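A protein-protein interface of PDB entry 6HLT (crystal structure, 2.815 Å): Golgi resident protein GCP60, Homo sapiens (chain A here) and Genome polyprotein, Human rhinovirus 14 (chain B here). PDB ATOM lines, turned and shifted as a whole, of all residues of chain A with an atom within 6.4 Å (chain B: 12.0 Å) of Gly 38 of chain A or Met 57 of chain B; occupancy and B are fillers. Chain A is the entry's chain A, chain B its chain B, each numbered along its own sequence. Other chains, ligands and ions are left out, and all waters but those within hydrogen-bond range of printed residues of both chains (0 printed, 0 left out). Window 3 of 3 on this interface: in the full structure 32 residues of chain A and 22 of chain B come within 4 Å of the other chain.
OE1 of Glu 39 of chain A lies within salt-bridge range of NH1 of Arg 55 of chain B (2.8 Å). The backbone NH (N) of Val 40 of chain A lies within hydrogen-bond range of the backbone carbonyl oxygen (O) of Ala 56 of chain B (3.2 Å). O of Met 57 of chain B sits close to O of Gly 38 of chain A (3.4 Å).
Met 57 of chain B touches just these residues of chain A: Gly 38 and Glu 39. Gly 36 of chain A touches just one residue of chain B: Arg 55 (3.9 Å). Of the printed residues of chain B, Val 40 of chain A touches Glu 54, Arg 55 and Ala 56. No residue of chain B comes within 4 Å of Asn 148 of chain A. No residue of chain B comes within 4 Å of Ser 151 of chain A. Of the printed residues of chain A, Ala 56 of chain B touches Glu 39 (3.3 Å) and Val 40 (3.2 Å). Of the printed residues of chain A, Arg 55 of chain B touches Gly 36, Glu 39 and Val 40. Of the printed residues of chain A, Glu 54 of chain B touches Val 40.
Of the 5 printed residues of chain B, 4 touch a printed residue of chain A. Hydrophobic or aromatic side chains of chain B that line the printed part of chain A: Met 57. Along chain B the printed residues that touch a printed residue of chain A span positions 54 to 57. Along chain A the printed residues that touch a printed residue of chain B span positions 36 to 40. Among the printed residues, Asp or Glu carboxylates within 4 Å of a Lys or Arg side-chain nitrogen of the other chain: Glu 39 of chain A with Arg 55 of chain B (2.8 Å).
Among the printed residues, pairs that only touch across the chains: Gly 36 of chain A with Arg 55 of chain B, Glu 39 of chain A with Ala 56 of chain B, Glu 39 of chain A with Met 57 of chain B, Val 40 of chain A with Glu 54 of chain B and Val 40 of chain A with Arg 55 of chain B.
The backbone NH (N) of Gly 36 of chain A lies within hydrogen-bond range of the side-chain carboxylate (OE1) of Glu 39 of chain A, 2.8 Å away. The backbone carbonyl oxygen (O) of Gly 36 of chain A is in hydrogen-bond range of the side-chain amide nitrogen (ND2) of Asn 148 of chain A (2.9 Å). The backbone NH (N) of Gly 38 of chain A sits at hydrogen-bond distance from the backbone carbonyl oxygen (O) of Ser 151 of chain A (3.1 Å). N of Asn 148 of chain A lies within hydrogen-bond range of O of Glu 39 of chain A (2.8 Å).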
ATOM      1  N   VAL A  35     -15.404  -3.196  14.459  1.00  0.00           N
ATOM      2  CA  VAL A  35     -16.721  -2.604  14.335  1.00  0.00           C
ATOM      3  C   VAL A  35     -16.597  -1.105  14.502  1.00  0.00           C
ATOM      4  O   VAL A  35     -16.181  -0.610  15.553  1.00  0.00           O
ATOM      5  CB  VAL A  35     -17.695  -3.170  15.366  1.00  0.00           C
ATOM      6  CG1 VAL A  35     -19.125  -2.724  15.048  1.00  0.00           C
ATOM      7  CG2 VAL A  35     -17.591  -4.688  15.390  1.00  0.00           C
ATOM      8  N   GLY A  36     -16.941  -0.391  13.440  1.00  0.00           N
ATOM      9  CA  GLY A  36     -16.869   1.050  13.439  1.00  0.00           C
ATOM     10  C   GLY A  36     -17.898   1.669  14.359  1.00  0.00           C
ATOM     11  O   GLY A  36     -18.754   0.985  14.923  1.00  0.00           O
ATOM     12  N   ARG A  37     -17.812   2.984  14.499  1.00  0.00           N
ATOM     13  CA  ARG A  37     -18.716   3.731  15.360  1.00  0.00           C
ATOM     14  C   ARG A  37     -20.129   3.684  14.777  1.00  0.00           C
ATOM     15  O   ARG A  37     -20.321   3.912  13.583  1.00  0.00           O
ATOM     16  CB  ARG A  37     -18.222   5.173  15.521  1.00  0.00           C
ATOM     17  CG  ARG A  37     -16.703   5.276  15.692  1.00  0.00           C
ATOM     18  CD  ARG A  37     -16.234   6.677  16.068  1.00  0.00           C
ATOM     19  NE  ARG A  37     -16.652   7.693  15.104  1.00  0.00           N
ATOM     20  CZ  ARG A  37     -16.205   8.948  15.094  1.00  0.00           C
ATOM     21  NH1 ARG A  37     -15.310   9.358  15.989  1.00  0.00           N
ATOM     22  NH2 ARG A  37     -16.653   9.795  14.179  1.00  0.00           N
ATOM     23  N   GLY A  38     -21.104   3.346  15.618  1.00  0.00           N
ATOM     24  CA  GLY A  38     -22.498   3.275  15.209  1.00  0.00           C
ATOM     25  C   GLY A  38     -22.829   2.153  14.240  1.00  0.00           C
ATOM     26  O   GLY A  38     -23.886   2.171  13.605  1.00  0.00           O
ATOM     27  N   GLU A  39     -21.945   1.159  14.157  1.00  0.00           N
ATOM     28  CA  GLU A  39     -22.088   0.054  13.213  1.00  0.00           C
ATOM     29  C   GLU A  39     -22.588  -1.234  13.854  1.00  0.00           C
ATOM     30  O   GLU A  39     -22.367  -1.478  15.039  1.00  0.00           O
ATOM     31  CB  GLU A  39     -20.758  -0.241  12.536  1.00  0.00           C
ATOM     32  CG  GLU A  39     -20.407   0.697  11.419  1.00  0.00           C
ATOM     33  CD  GLU A  39     -19.152   0.264  10.700  1.00  0.00           C
ATOM     34  OE1 GLU A  39     -18.538  -0.735  11.139  1.00  0.00           O
ATOM     35  OE2 GLU A  39     -18.781   0.916   9.702  1.00  0.00           O
ATOM     36  N   VAL A  40     -23.298  -2.030  13.057  1.00  0.00           N
ATOM     37  CA  VAL A  40     -23.676  -3.384  13.438  1.00  0.00           C
ATOM     38  C   VAL A  40     -23.104  -4.380  12.429  1.00  0.00           C
ATOM     39  O   VAL A  40     -23.524  -4.409  11.271  1.00  0.00           O
ATOM     40  CB  VAL A  40     -25.213  -3.563  13.515  1.00  0.00           C
ATOM     41  CG1 VAL A  40     -25.574  -4.972  13.976  1.00  0.00           C
ATOM     42  CG2 VAL A  40     -25.825  -2.562  14.461  1.00  0.00           C
ATOM     43  N   ASN A 148     -22.565  -2.218  17.720  1.00  0.00           N
ATOM     44  CA  ASN A 148     -21.926  -1.016  18.256  1.00  0.00           C
ATOM     45  C   ASN A 148     -22.783   0.251  18.125  1.00  0.00           C
ATOM     46  O   ASN A 148     -22.287   1.347  18.378  1.00  0.00           O
ATOM     47  CB  ASN A 148     -20.574  -0.787  17.579  1.00  0.00           C
ATOM     48  CG  ASN A 148     -19.610   0.008  18.449  1.00  0.00           C
ATOM     49  OD1 ASN A 148     -19.799   0.129  19.659  1.00  0.00           O
ATOM     50  ND2 ASN A 148     -18.568   0.555  17.830  1.00  0.00           N
ATOM     51  N   SER A 149     -24.033   0.103  17.685  1.00  0.00           N
ATOM     52  CA  SER A 149     -24.904   1.239  17.343  1.00  0.00           C
ATOM     53  C   SER A 149     -24.904   2.371  18.361  1.00  0.00           C
ATOM     54  O   SER A 149     -24.927   3.546  17.995  1.00  0.00           O
ATOM     55  CB  SER A 149     -26.346   0.767  17.183  1.00  0.00           C
ATOM     56  OG  SER A 149     -26.452  -0.229  16.190  1.00  0.00           O
ATOM     57  N   TYR A 150     -24.898   2.004  19.636  1.00  0.00           N
ATOM     58  CA  TYR A 150     -24.971   2.972  20.720  1.00  0.00           C
ATOM     59  C   TYR A 150     -23.729   3.861  20.767  1.00  0.00           C
ATOM     60  O   TYR A 150     -23.821   5.042  21.097  1.00  0.00           O
ATOM     61  CB  TYR A 150     -25.164   2.247  22.063  1.00  0.00           C
ATOM     62  CG  TYR A 150     -24.036   1.307  22.448  1.00  0.00           C
ATOM     63  CD1 TYR A 150     -24.032  -0.019  22.033  1.00  0.00           C
ATOM     64  CD2 TYR A 150     -22.977   1.747  23.230  1.00  0.00           C
ATOM     65  CE1 TYR A 150     -23.001  -0.876  22.380  1.00  0.00           C
ATOM     66  CE2 TYR A 150     -21.941   0.897  23.581  1.00  0.00           C
ATOM     67  CZ  TYR A 150     -21.960  -0.411  23.155  1.00  0.00           C
ATOM     68  OH  TYR A 150     -20.931  -1.252  23.512  1.00  0.00           O
ATOM     69  N   SER A 151     -22.573   3.302  20.423  1.00  0.00           N
ATOM     70  CA  SER A 151     -21.311   4.009  20.622  1.00  0.00           C
ATOM     71  C   SER A 151     -21.067   5.085  19.584  1.00  0.00           C
ATOM     72  O   SER A 151     -20.937   4.797  18.399  1.00  0.00           O
ATOM     73  CB  SER A 151     -20.134   3.042  20.589  1.00  0.00           C
ATOM     74  OG  SER A 151     -18.910   3.760  20.626  1.00  0.00           O
ATOM     75  N   LEU A 152     -20.955   6.322  20.049  1.00  0.00           N
ATOM     76  CA  LEU A 152     -20.687   7.439  19.162  1.00  0.00           C
ATOM     77  C   LEU A 152     -19.229   7.565  18.763  1.00  0.00           C
ATOM     78  O   LEU A 152     -18.919   7.764  17.594  1.00  0.00           O
ATOM     79  CB  LEU A 152     -21.127   8.736  19.824  1.00  0.00           C
ATOM     80  CG  LEU A 152     -22.617   8.813  20.146  1.00  0.00           C
ATOM     81  CD1 LEU A 152     -22.877  10.025  21.010  1.00  0.00           C
ATOM     82  CD2 LEU A 152     -23.447   8.856  18.865  1.00  0.00           C
ATOM     83  N   ARG A 154     -16.390   5.424  19.685  1.00  0.00           N
ATOM     84  CA  ARG A 154     -15.454   4.316  19.932  1.00  0.00           C
ATOM     85  C   ARG A 154     -15.654   3.106  19.026  1.00  0.00           C
ATOM     86  O   ARG A 154     -16.700   2.464  19.062  1.00  0.00           O
ATOM     87  CB  ARG A 154     -15.566   3.854  21.391  1.00  0.00           C
ATOM     88  CG  ARG A 154     -15.480   4.970  22.432  1.00  0.00           C
ATOM     89  CD  ARG A 154     -14.074   5.532  22.548  1.00  0.00           C
ATOM     90  NE  ARG A 154     -14.033   6.745  23.364  1.00  0.00           N
ATOM     91  CZ  ARG A 154     -12.917   7.308  23.820  1.00  0.00           C
ATOM     92  NH1 ARG A 154     -11.733   6.769  23.553  1.00  0.00           N
ATOM     93  NH2 ARG A 154     -12.981   8.411  24.553  1.00  0.00           N
ATOM     94  N   ILE B  53     -20.187 -11.513   5.978  1.00  0.00           N
ATOM     95  CA  ILE B  53     -20.097 -10.613   7.096  1.00  0.00           C
ATOM     96  C   ILE B  53     -20.577  -9.252   6.624  1.00  0.00           C
ATOM     97  O   ILE B  53     -19.900  -8.563   5.861  1.00  0.00           O
ATOM     98  CB  ILE B  53     -18.672 -10.576   7.650  1.00  0.00           C
ATOM     99  CG1 ILE B  53     -18.258 -12.012   8.018  1.00  0.00           C
ATOM    100  CG2 ILE B  53     -18.597  -9.620   8.835  1.00  0.00           C
ATOM    101  CD1 ILE B  53     -16.991 -12.134   8.832  1.00  0.00           C
ATOM    102  N   GLU B  54     -21.743  -8.867   7.137  1.00  0.00           N
ATOM    103  CA  GLU B  54     -22.494  -7.716   6.649  1.00  0.00           C
ATOM    104  C   GLU B  54     -22.221  -6.542   7.577  1.00  0.00           C
ATOM    105  O   GLU B  54     -21.920  -6.742   8.754  1.00  0.00           O
ATOM    106  CB  GLU B  54     -24.001  -8.028   6.582  1.00  0.00           C
ATOM    107  CG  GLU B  54     -24.320  -9.448   6.103  1.00  0.00           C
ATOM    108  CD  GLU B  54     -25.812  -9.696   5.854  1.00  0.00           C
ATOM    109  OE1 GLU B  54     -26.161 -10.080   4.711  1.00  0.00           O
ATOM    110  OE2 GLU B  54     -26.627  -9.529   6.793  1.00  0.00           O
ATOM    111  N   ARG B  55     -22.254  -5.332   7.022  1.00  0.00           N
ATOM    112  CA  ARG B  55     -22.017  -4.109   7.787  1.00  0.00           C
ATOM    113  C   ARG B  55     -23.151  -3.094   7.559  1.00  0.00           C
ATOM    114  O   ARG B  55     -23.513  -2.809   6.415  1.00  0.00           O
ATOM    115  CB  ARG B  55     -20.669  -3.502   7.394  1.00  0.00           C
ATOM    116  CG  ARG B  55     -19.933  -2.804   8.526  1.00  0.00           C
ATOM    117  CD  ARG B  55     -18.558  -2.331   8.077  1.00  0.00           C
ATOM    118  NE  ARG B  55     -17.553  -3.387   8.207  1.00  0.00           N
ATOM    119  CZ  ARG B  55     -16.730  -3.535   9.245  1.00  0.00           C
ATOM    120  NH1 ARG B  55     -16.756  -2.694  10.270  1.00  0.00           N
ATOM    121  NH2 ARG B  55     -15.864  -4.535   9.257  1.00  0.00           N
ATOM    122  N   ALA B  56     -23.696  -2.555   8.650  1.00  0.00           N
ATOM    123  CA  ALA B  56     -24.822  -1.618   8.595  1.00  0.00           C
ATOM    124  C   ALA B  56     -24.557  -0.413   9.497  1.00  0.00           C
ATOM    125  O   ALA B  56     -23.617  -0.432  10.289  1.00  0.00           O
ATOM    126  CB  ALA B  56     -26.118  -2.317   8.999  1.00  0.00           C
ATOM    127  N   MET B  57     -25.377   0.631   9.361  1.00  0.00           N
ATOM    128  CA  MET B  57     -25.265   1.832  10.194  1.00  0.00           C
ATOM    129  C   MET B  57     -26.576   2.152  10.913  1.00  0.00           C
ATOM    130  O   MET B  57     -26.637   3.065  11.744  1.00  0.00           O
ATOM    131  CB  MET B  57     -24.844   3.022   9.340  1.00  0.00           C
ATOM    132  CG  MET B  57     -23.447   2.900   8.766  1.00  0.00           C
ATOM    133  SD  MET B  57     -22.183   3.534   9.883  1.00  0.00           S
ATOM    134  CE  MET B  57     -20.739   3.397   8.832  1.00  0.00           C
